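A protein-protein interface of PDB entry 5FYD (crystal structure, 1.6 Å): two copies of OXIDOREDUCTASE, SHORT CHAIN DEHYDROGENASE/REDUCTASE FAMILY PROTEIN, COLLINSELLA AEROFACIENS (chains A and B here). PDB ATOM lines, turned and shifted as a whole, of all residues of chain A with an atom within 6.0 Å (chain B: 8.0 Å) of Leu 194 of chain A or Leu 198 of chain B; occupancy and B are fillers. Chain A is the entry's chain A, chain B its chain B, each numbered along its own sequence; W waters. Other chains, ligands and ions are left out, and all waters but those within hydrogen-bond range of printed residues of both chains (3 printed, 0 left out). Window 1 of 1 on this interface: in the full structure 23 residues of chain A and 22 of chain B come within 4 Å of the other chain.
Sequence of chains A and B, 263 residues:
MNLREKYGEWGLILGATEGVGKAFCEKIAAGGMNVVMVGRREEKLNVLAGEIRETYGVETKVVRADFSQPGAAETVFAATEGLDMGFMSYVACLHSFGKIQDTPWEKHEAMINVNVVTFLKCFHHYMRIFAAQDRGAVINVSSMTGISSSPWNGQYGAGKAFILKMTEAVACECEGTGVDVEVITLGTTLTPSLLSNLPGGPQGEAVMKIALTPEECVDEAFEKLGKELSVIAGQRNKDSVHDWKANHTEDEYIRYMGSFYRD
The side-chain amide oxygen of Asn 197 of chain B sits at hydrogen-bond distance from the side-chain hydroxyl of Ser 193 of chain A, at 2.9 Å. The side-chain amide oxygen (OD1) of Asn 197 of chain A lies within hydrogen-bond range of the side-chain hydroxyl (OG) of Ser 193 of chain B (2.6 Å). The backbone NH (N) of Gly 200 of chain B is in hydrogen-bond range of the side-chain hydroxyl (OG1) of Thr 188 of chain A (3.1 Å). OG1 of Thr 188 of chain A is in hydrogen-bond range of O of Gly 201 of chain B (2.7 Å).
The side-chain hydroxyl of Ser 196 of chain B lies within hydrogen-bond range of the side-chain amide nitrogen of Asn 197 of chain B (3.2 Å). The backbone carbonyl oxygen (O) of Ser 193 of chain A lies within hydrogen-bond range of the side-chain amide nitrogen (ND2) of Asn 197 of chain A (2.7 Å). The backbone NH (N) of Ser 193 of chain B sits close to the side-chain hydroxyl (OG1) of Thr 191 of chain B, 3.4 Å away. The backbone carbonyl oxygen (O) of Ser 193 of chain A is in hydrogen-bond range of the side-chain hydroxyl (OG) of Ser 196 of chain A (3.1 Å). The backbone NH of Leu 194 of chain A sits at hydrogen-bond distance from the side-chain hydroxyl of Thr 191 of chain A. OG1 of Thr 191 of chain B sits at hydrogen-bond distance from N of Leu 194 of chain B (3.2 Å).
Among the printed residues, pairs that only touch across the chains: Ile 210 of chain A with Gly 201 of chain B (3.0 Å), Leu 198 of chain A with Thr 188 of chain B (3.3 Å), Thr 188 of chain A with Leu 198 of chain B (3.3 Å), Asn 197 of chain A with Thr 188 of chain B (3.5 Å), Leu 194 of chain A with Asn 197 of chain B (3.5 Å), Thr 188 of chain A with Pro 199 of chain B (3.5 Å), Thr 188 of chain A with Asn 197 of chain B (3.6 Å), Met 257 of chain A with Gln 203 of chain B (3.7 Å), Asn 197 of chain A with Leu 194 of chain B (3.7 Å), Gly 187 of chain A with Pro 199 of chain B (3.7 Å), Gly 187 of chain A with Gly 200 of chain B (3.7 Å), Ile 210 of chain A with Pro 202 of chain B (3.8 Å), Leu 194 of chain A with Leu 198 of chain B (3.8 Å) and Val 207 of chain A with Leu 198 of chain B (3.9 Å).
Leu 194 of chain A touches just these residues of chain B: Asn 197 and Leu 198. Of chain A, only Thr 188 (3.3 Å), Leu 194 (3.8 Å) and Val 207 (3.9 Å) come within 4 Å of Leu 198 of chain B. Printed residues of chain A within 4 Å of Gly 201 of chain B: Thr 188 (2.7 Å) and Ile 210 (3.0 Å). Printed residues of chain B within 4 Å of Ile 210 of chain A: Gly 201 and Pro 202. Of the printed residues of chain A, Asn 197 of chain B touches Thr 188 (3.6 Å), Ser 193 (2.9 Å) and Leu 194 (3.5 Å). Of the printed residues of chain B, Thr 188 of chain A touches Asn 197, Leu 198, Pro 199, Gly 200 and Gly 201. Ser 196 of chain A touches none of the printed residues of chain B. Thr 189 of chain B touches none of the printed residues of chain A. The nearest residue of chain B that does not touch Leu 194 of chain A is Leu 194 of chain B (4.7 Å). The nearest printed residue of chain B that does not touch Ser 193 of chain A is Ser 193 of chain B (6.0 Å).
Of the 16 printed residues of chain B, 10 touch a printed residue of chain A. Hydrophobic or aromatic side chains of chain B within 4 Å of the printed part of chain A: Leu 194, Leu 198, Pro 199 and Pro 202. Along chain B the printed residues that touch a printed residue of chain A span positions 188 to 203. Of the 16 printed residues of chain A, 9 touch a printed residue of chain B. Along chain A the printed residues that touch a printed residue of chain B span positions 187 to 257.
Thr 188 of chain A touches Asn 197 of chain B, and with the chains exchanged Asn 197 of chain A touches Thr 188 of chain B. Thr 188 of chain A touches Leu 198 of chain B, and with the chains exchanged Leu 198 of chain A touches Thr 188 of chain B. Leu 194 of chain A touches Asn 197 of chain B, and with the chains exchanged Asn 197 of chain A touches Leu 194 of chain B. Leu 194 of chain A touches Leu 198 of chain B, but with the chains exchanged Leu 198 of chain A does not touch Leu 194 of chain B (4.05 Å). Positions printed for both chains: 188, 189, 190, 191, 192, 193, 194, 195, 196, 197 and 198.
Water W1 lies within hydrogen-bond range of the backbone NH (N) of Thr 188 of chain A (2.9 Å), the backbone carbonyl oxygen (O) of Ile 210 of chain A (3.1 Å) and the backbone carbonyl oxygen (O) of Gly 200 of chain B (3.3 Å). Water W2 lies within hydrogen-bond range of the backbone NH of Thr 189 of chain A and the backbone carbonyl oxygen of Asn 197 of chain B. Water W3 lies within hydrogen-bond range of O of Asn 197 of chain A (2.9 Å) and N of Thr 189 of chain B (3.1 Å).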
ATOM      1  N   GLY A 187       3.481  19.044  19.381  1.00  0.00           N
ATOM      2  CA  GLY A 187       4.415  20.007  19.891  1.00  0.00           C
ATOM      3  C   GLY A 187       4.125  20.141  21.372  1.00  0.00           C
ATOM      4  O   GLY A 187       3.729  19.194  22.046  1.00  0.00           O
ATOM      5  N   THR A 188       4.271  21.346  21.873  1.00  0.00           N
ATOM      6  CA  THR A 188       4.001  21.611  23.273  1.00  0.00           C
ATOM      7  C   THR A 188       2.503  21.482  23.547  1.00  0.00           C
ATOM      8  O   THR A 188       1.683  22.060  22.837  1.00  0.00           O
ATOM      9  CB  THR A 188       4.564  22.987  23.628  1.00  0.00           C
ATOM     10  OG1 THR A 188       5.961  22.970  23.311  1.00  0.00           O
ATOM     11  CG2 THR A 188       4.345  23.317  25.079  1.00  0.00           C
ATOM     12  N   THR A 189       2.177  20.653  24.529  1.00  0.00           N
ATOM     13  CA  THR A 189       0.819  20.249  24.821  1.00  0.00           C
ATOM     14  C   THR A 189       0.519  20.581  26.287  1.00  0.00           C
ATOM     15  O   THR A 189       1.369  20.401  27.149  1.00  0.00           O
ATOM     16  CB  THR A 189       0.654  18.735  24.593  1.00  0.00           C
ATOM     17  OG1 THR A 189       1.042  18.398  23.243  1.00  0.00           O
ATOM     18  CG2 THR A 189      -0.775  18.306  24.843  1.00  0.00           C
ATOM     19  N   LEU A 190      -0.682  21.073  26.542  1.00  0.00           N
ATOM     20  CA  LEU A 190      -1.094  21.453  27.893  1.00  0.00           C
ATOM     21  C   LEU A 190      -1.319  20.194  28.729  1.00  0.00           C
ATOM     22  O   LEU A 190      -2.252  19.436  28.489  1.00  0.00           O
ATOM     23  CB  LEU A 190      -2.359  22.293  27.825  1.00  0.00           C
ATOM     24  CG  LEU A 190      -2.961  22.852  29.123  1.00  0.00           C
ATOM     25  CD1 LEU A 190      -2.066  23.922  29.724  1.00  0.00           C
ATOM     26  CD2 LEU A 190      -4.343  23.409  28.833  1.00  0.00           C
ATOM     27  N   THR A 191      -0.414  19.961  29.671  1.00  0.00           N
ATOM     28  CA  THR A 191      -0.486  18.851  30.613  1.00  0.00           C
ATOM     29  C   THR A 191      -0.301  19.423  32.027  1.00  0.00           C
ATOM     30  O   THR A 191       0.023  20.619  32.174  1.00  0.00           O
ATOM     31  CB  THR A 191       0.596  17.802  30.293  1.00  0.00           C
ATOM     32  OG1 THR A 191       1.893  18.411  30.318  1.00  0.00           O
ATOM     33  CG2 THR A 191       0.364  17.195  28.909  1.00  0.00           C
ATOM     34  N   PRO A 192      -0.531  18.595  33.073  1.00  0.00           N
ATOM     35  CA  PRO A 192      -0.150  19.051  34.421  1.00  0.00           C
ATOM     36  C   PRO A 192       1.371  19.128  34.551  1.00  0.00           C
ATOM     37  O   PRO A 192       1.886  20.010  35.237  1.00  0.00           O
ATOM     38  CB  PRO A 192      -0.741  17.984  35.361  1.00  0.00           C
ATOM     39  CG  PRO A 192      -1.538  17.049  34.507  1.00  0.00           C
ATOM     40  CD  PRO A 192      -1.106  17.233  33.086  1.00  0.00           C
ATOM     41  N   SER A 193       2.061  18.185  33.906  1.00  0.00           N
ATOM     42  CA  SER A 193       3.503  18.265  33.652  1.00  0.00           C
ATOM     43  C   SER A 193       3.917  19.693  33.252  1.00  0.00           C
ATOM     44  O   SER A 193       4.798  20.283  33.886  1.00  0.00           O
ATOM     45  CB  SER A 193       3.909  17.264  32.554  1.00  0.00           C
ATOM     46  OG  SER A 193       5.165  16.677  32.823  1.00  0.00           O
ATOM     47  N   LEU A 194       3.252  20.249  32.231  1.00  0.00           N
ATOM     48  CA  LEU A 194       3.570  21.591  31.742  1.00  0.00           C
ATOM     49  C   LEU A 194       3.165  22.676  32.736  1.00  0.00           C
ATOM     50  O   LEU A 194       4.014  23.462  33.142  1.00  0.00           O
ATOM     51  CB  LEU A 194       2.923  21.873  30.378  1.00  0.00           C
ATOM     52  CG  LEU A 194       3.247  23.241  29.761  1.00  0.00           C
ATOM     53  CD1 LEU A 194       4.748  23.413  29.568  1.00  0.00           C
ATOM     54  CD2 LEU A 194       2.500  23.435  28.449  1.00  0.00           C
ATOM     55  N   LEU A 195       1.887  22.702  33.127  1.00  0.00           N
ATOM     56  CA  LEU A 195       1.337  23.766  33.988  1.00  0.00           C
ATOM     57  C   LEU A 195       2.082  23.945  35.313  1.00  0.00           C
ATOM     58  O   LEU A 195       2.218  25.075  35.787  1.00  0.00           O
ATOM     59  CB  LEU A 195      -0.151  23.539  34.278  1.00  0.00           C
ATOM     60  CG  LEU A 195      -1.129  23.874  33.152  1.00  0.00           C
ATOM     61  CD1 LEU A 195      -2.518  23.353  33.501  1.00  0.00           C
ATOM     62  CD2 LEU A 195      -1.170  25.368  32.865  1.00  0.00           C
ATOM     63  N   SER A 196       2.581  22.845  35.876  1.00  0.00           N
ATOM     64  CA  SER A 196       3.368  22.878  37.114  1.00  0.00           C
ATOM     65  C   SER A 196       4.804  23.386  36.934  1.00  0.00           C
ATOM     66  O   SER A 196       5.519  23.543  37.918  1.00  0.00           O
ATOM     67  CB  SER A 196       3.413  21.490  37.757  1.00  0.00           C
ATOM     68  OG  SER A 196       4.161  20.589  36.955  1.00  0.00           O
ATOM     69  N   ASN A 197       5.241  23.574  35.686  1.00  0.00           N
ATOM     70  CA  ASN A 197       6.452  24.338  35.374  1.00  0.00           C
ATOM     71  C   ASN A 197       6.126  25.741  34.834  1.00  0.00           C
ATOM     72  O   ASN A 197       7.023  26.426  34.342  1.00  0.00           O
ATOM     73  CB  ASN A 197       7.319  23.573  34.365  1.00  0.00           C
ATOM     74  CG  ASN A 197       7.921  22.302  34.948  1.00  0.00           C
ATOM     75  OD1 ASN A 197       9.076  22.297  35.372  1.00  0.00           O
ATOM     76  ND2 ASN A 197       7.146  21.221  34.964  1.00  0.00           N
ATOM     77  N   LEU A 198       4.869  26.184  34.955  1.00  0.00           N
ATOM     78  CA  LEU A 198       4.455  27.532  34.535  1.00  0.00           C
ATOM     79  C   LEU A 198       3.863  28.337  35.699  1.00  0.00           C
ATOM     80  O   LEU A 198       2.798  28.946  35.548  1.00  0.00           O
ATOM     81  CB  LEU A 198       3.436  27.470  33.385  1.00  0.00           C
ATOM     82  CG  LEU A 198       3.902  26.848  32.065  1.00  0.00           C
ATOM     83  CD1 LEU A 198       2.729  26.822  31.101  1.00  0.00           C
ATOM     84  CD2 LEU A 198       5.075  27.617  31.460  1.00  0.00           C
ATOM     85  N   VAL A 207       3.397  30.637  26.409  1.00  0.00           N
ATOM     86  CA  VAL A 207       3.371  29.209  26.084  1.00  0.00           C
ATOM     87  C   VAL A 207       1.998  28.753  25.537  1.00  0.00           C
ATOM     88  O   VAL A 207       1.961  27.901  24.646  1.00  0.00           O
ATOM     89  CB  VAL A 207       3.847  28.350  27.295  1.00  0.00           C
ATOM     90  CG1 VAL A 207       3.638  26.854  27.059  1.00  0.00           C
ATOM     91  CG2 VAL A 207       5.321  28.624  27.586  1.00  0.00           C
ATOM     92  N   ILE A 210       0.991  28.856  21.750  1.00  0.00           N
ATOM     93  CA  ILE A 210       1.447  27.714  20.949  1.00  0.00           C
ATOM     94  C   ILE A 210       1.278  26.334  21.608  1.00  0.00           C
ATOM     95  O   ILE A 210       1.791  25.345  21.073  1.00  0.00           O
ATOM     96  CB  ILE A 210       2.915  27.919  20.478  1.00  0.00           C
ATOM     97  CG1 ILE A 210       3.901  28.014  21.656  1.00  0.00           C
ATOM     98  CG2 ILE A 210       3.017  29.171  19.610  1.00  0.00           C
ATOM     99  CD1 ILE A 210       4.449  26.691  22.143  1.00  0.00           C
ATOM    100  N   ALA A 211       0.580  26.248  22.745  1.00  0.00           N
ATOM    101  CA  ALA A 211       0.228  24.944  23.332  1.00  0.00           C
ATOM    102  C   ALA A 211      -1.175  24.521  22.926  1.00  0.00           C
ATOM    103  O   ALA A 211      -2.104  25.327  22.924  1.00  0.00           O
ATOM    104  CB  ALA A 211       0.345  24.966  24.845  1.00  0.00           C
ATOM    105  N   MET A 257      17.426  24.391  18.694  1.00  0.00           N
ATOM    106  CA  MET A 257      17.019  23.507  19.777  1.00  0.00           C
ATOM    107  C   MET A 257      18.029  23.434  20.905  1.00  0.00           C
ATOM    108  O   MET A 257      17.642  23.366  22.063  1.00  0.00           O
ATOM    109  CB  MET A 257      16.732  22.095  19.271  1.00  0.00           C
ATOM    110  CG  MET A 257      15.581  22.001  18.282  1.00  0.00           C
ATOM    111  SD  MET A 257      14.009  22.636  18.911  1.00  0.00           S
ATOM    112  CE  MET A 257      13.730  21.557  20.305  1.00  0.00           C
ATOM    113  N   THR B 188       7.893  31.724  35.987  1.00  0.00           N
ATOM    114  CA  THR B 188       8.432  30.626  35.180  1.00  0.00           C
ATOM    115  C   THR B 188       9.913  30.856  34.870  1.00  0.00           C
ATOM    116  O   THR B 188      10.285  31.906  34.358  1.00  0.00           O
ATOM    117  CB  THR B 188       7.631  30.508  33.889  1.00  0.00           C
ATOM    118  OG1 THR B 188       6.261  30.267  34.224  1.00  0.00           O
ATOM    119  CG2 THR B 188       8.170  29.407  32.974  1.00  0.00           C
ATOM    120  N   THR B 189      10.746  29.876  35.206  1.00  0.00           N
ATOM    121  CA  THR B 189      12.188  30.006  35.066  1.00  0.00           C
ATOM    122  C   THR B 189      12.729  28.956  34.088  1.00  0.00           C
ATOM    123  O   THR B 189      12.228  27.828  34.044  1.00  0.00           O
ATOM    124  CB  THR B 189      12.884  29.875  36.429  1.00  0.00           C
ATOM    125  OG1 THR B 189      12.766  28.534  36.888  1.00  0.00           O
ATOM    126  CG2 THR B 189      12.229  30.813  37.475  1.00  0.00           C
ATOM    127  N   LEU B 190      13.742  29.353  33.322  1.00  0.00           N
ATOM    128  CA  LEU B 190      14.367  28.496  32.302  1.00  0.00           C
ATOM    129  C   LEU B 190      15.211  27.399  32.954  1.00  0.00           C
ATOM    130  O   LEU B 190      16.355  27.647  33.341  1.00  0.00           O
ATOM    131  CB  LEU B 190      15.242  29.325  31.348  1.00  0.00           C
ATOM    132  CG  LEU B 190      14.531  30.158  30.279  1.00  0.00           C
ATOM    133  CD1 LEU B 190      15.433  31.246  29.698  1.00  0.00           C
ATOM    134  CD2 LEU B 190      14.014  29.255  29.160  1.00  0.00           C
ATOM    135  N   THR B 191      14.632  26.203  33.083  1.00  0.00           N
ATOM    136  CA  THR B 191      15.322  25.030  33.630  1.00  0.00           C
ATOM    137  C   THR B 191      15.168  23.827  32.679  1.00  0.00           C
ATOM    138  O   THR B 191      14.258  23.811  31.845  1.00  0.00           O
ATOM    139  CB  THR B 191      14.742  24.611  34.980  1.00  0.00           C
ATOM    140  OG1 THR B 191      13.423  24.089  34.788  1.00  0.00           O
ATOM    141  CG2 THR B 191      14.693  25.799  35.934  1.00  0.00           C
ATOM    142  N   PRO B 192      16.032  22.802  32.825  1.00  0.00           N
ATOM    143  CA  PRO B 192      15.860  21.596  31.997  1.00  0.00           C
ATOM    144  C   PRO B 192      14.466  20.987  32.111  1.00  0.00           C
ATOM    145  O   PRO B 192      13.907  20.523  31.114  1.00  0.00           O
ATOM    146  CB  PRO B 192      16.919  20.640  32.564  1.00  0.00           C
ATOM    147  CG  PRO B 192      17.990  21.545  33.048  1.00  0.00           C
ATOM    148  CD  PRO B 192      17.241  22.698  33.672  1.00  0.00           C
ATOM    149  N   SER B 193      13.919  21.013  33.324  1.00  0.00           N
ATOM    150  CA  SER B 193      12.569  20.546  33.600  1.00  0.00           C
ATOM    151  C   SER B 193      11.500  21.290  32.765  1.00  0.00           C
ATOM    152  O   SER B 193      10.570  20.662  32.258  1.00  0.00           O
ATOM    153  CB  SER B 193      12.289  20.662  35.110  1.00  0.00           C
ATOM    154  OG  SER B 193      10.913  20.521  35.413  1.00  0.00           O
ATOM    155  N   LEU B 194      11.627  22.607  32.616  1.00  0.00           N
ATOM    156  CA  LEU B 194      10.700  23.362  31.750  1.00  0.00           C
ATOM    157  C   LEU B 194      10.923  23.000  30.276  1.00  0.00           C
ATOM    158  O   LEU B 194       9.970  22.704  29.552  1.00  0.00           O
ATOM    159  CB  LEU B 194      10.842  24.874  31.942  1.00  0.00           C
ATOM    160  CG  LEU B 194      10.074  25.780  30.967  1.00  0.00           C
ATOM    161  CD1 LEU B 194       8.568  25.607  31.106  1.00  0.00           C
ATOM    162  CD2 LEU B 194      10.497  27.226  31.176  1.00  0.00           C
ATOM    163  N   LEU B 195      12.178  23.032  29.846  1.00  0.00           N
ATOM    164  CA  LEU B 195      12.518  22.818  28.439  1.00  0.00           C
ATOM    165  C   LEU B 195      12.120  21.434  27.927  1.00  0.00           C
ATOM    166  O   LEU B 195      11.723  21.307  26.765  1.00  0.00           O
ATOM    167  CB  LEU B 195      14.010  23.039  28.201  1.00  0.00           C
ATOM    168  CG  LEU B 195      14.537  24.465  28.332  1.00  0.00           C
ATOM    169  CD1 LEU B 195      16.063  24.451  28.289  1.00  0.00           C
ATOM    170  CD2 LEU B 195      13.963  25.370  27.254  1.00  0.00           C
ATOM    171  N   SER B 196      12.215  20.417  28.785  1.00  0.00           N
ATOM    172  CA  SER B 196      11.733  19.080  28.444  1.00  0.00           C
ATOM    173  C   SER B 196      10.222  19.045  28.202  1.00  0.00           C
ATOM    174  O   SER B 196       9.751  18.182  27.480  1.00  0.00           O
ATOM    175  CB  SER B 196      12.129  18.061  29.518  1.00  0.00           C
ATOM    176  OG  SER B 196      11.534  18.375  30.763  1.00  0.00           O
ATOM    177  N   ASN B 197       9.470  19.977  28.791  1.00  0.00           N
ATOM    178  CA  ASN B 197       8.010  20.103  28.553  1.00  0.00           C
ATOM    179  C   ASN B 197       7.633  21.086  27.441  1.00  0.00           C
ATOM    180  O   ASN B 197       6.447  21.423  27.281  1.00  0.00           O
ATOM    181  CB  ASN B 197       7.302  20.502  29.849  1.00  0.00           C
ATOM    182  CG  ASN B 197       7.342  19.403  30.887  1.00  0.00           C
ATOM    183  OD1 ASN B 197       6.331  18.761  31.156  1.00  0.00           O
ATOM    184  ND2 ASN B 197       8.514  19.174  31.467  1.00  0.00           N
ATOM    185  N   LEU B 198       8.619  21.543  26.670  1.00  0.00           N
ATOM    186  CA  LEU B 198       8.381  22.439  25.547  1.00  0.00           C
ATOM    187  C   LEU B 198       8.943  21.833  24.264  1.00  0.00           C
ATOM    188  O   LEU B 198       9.752  22.466  23.572  1.00  0.00           O
ATOM    189  CB  LEU B 198       9.008  23.820  25.814  1.00  0.00           C
ATOM    190  CG  LEU B 198       8.450  24.595  27.010  1.00  0.00           C
ATOM    191  CD1 LEU B 198       9.253  25.867  27.206  1.00  0.00           C
ATOM    192  CD2 LEU B 198       6.973  24.920  26.836  1.00  0.00           C
ATOM    193  N   PRO B 199       8.485  20.611  23.911  1.00  0.00           N
ATOM    194  CA  PRO B 199       9.051  19.948  22.720  1.00  0.00           C
ATOM    195  C   PRO B 199       8.836  20.686  21.408  1.00  0.00           C
ATOM    196  O   PRO B 199       9.673  20.572  20.512  1.00  0.00           O
ATOM    197  CB  PRO B 199       8.337  18.591  22.698  1.00  0.00           C
ATOM    198  CG  PRO B 199       7.093  18.780  23.492  1.00  0.00           C
ATOM    199  CD  PRO B 199       7.465  19.772  24.562  1.00  0.00           C
ATOM    200  N   GLY B 200       7.736  21.428  21.293  1.00  0.00           N
ATOM    201  CA  GLY B 200       7.437  22.194  20.087  1.00  0.00           C
ATOM    202  C   GLY B 200       7.649  23.686  20.199  1.00  0.00           C
ATOM    203  O   GLY B 200       7.122  24.443  19.374  1.00  0.00           O
ATOM    204  N   GLY B 201       8.428  24.117  21.198  1.00  0.00           N
ATOM    205  CA  GLY B 201       8.692  25.542  21.437  1.00  0.00           C
ATOM    206  C   GLY B 201       7.868  26.143  22.576  1.00  0.00           C
ATOM    207  O   GLY B 201       7.033  25.446  23.174  1.00  0.00           O
ATOM    208  N   PRO B 202       8.121  27.414  22.924  1.00  0.00           N
ATOM    209  CA  PRO B 202       9.274  28.177  22.416  1.00  0.00           C
ATOM    210  C   PRO B 202      10.576  27.577  22.949  1.00  0.00           C
ATOM    211  O   PRO B 202      10.590  27.027  24.058  1.00  0.00           O
ATOM    212  CB  PRO B 202       9.043  29.579  22.982  1.00  0.00           C
ATOM    213  CG  PRO B 202       8.315  29.331  24.258  1.00  0.00           C
ATOM    214  CD  PRO B 202       7.409  28.154  23.986  1.00  0.00           C
ATOM    215  N   GLN B 203      11.632  27.639  22.137  1.00  0.00           N
ATOM    216  CA  GLN B 203      12.927  27.038  22.459  1.00  0.00           C
ATOM    217  C   GLN B 203      14.040  28.011  22.067  1.00  0.00           C
ATOM    218  O   GLN B 203      13.760  29.052  21.467  1.00  0.00           O
ATOM    219  CB  GLN B 203      13.086  25.703  21.715  1.00  0.00           C
ATOM    220  CG  GLN B 203      12.311  24.530  22.327  1.00  0.00           C
ATOM    221  CD  GLN B 203      13.077  23.780  23.415  1.00  0.00           C
ATOM    222  OE1 GLN B 203      14.307  23.851  23.492  1.00  0.00           O
ATOM    223  NE2 GLN B 203      12.350  23.050  24.256  1.00  0.00           N
HETATM  224  O   HOH W   1       4.072  23.523  20.035  1.00  0.00           O
HETATM  225  O   HOH W   2       4.347  19.696  26.201  1.00  0.00           O
HETATM  226  O   HOH W   3       9.253  27.318  35.983  1.00  0.00           O
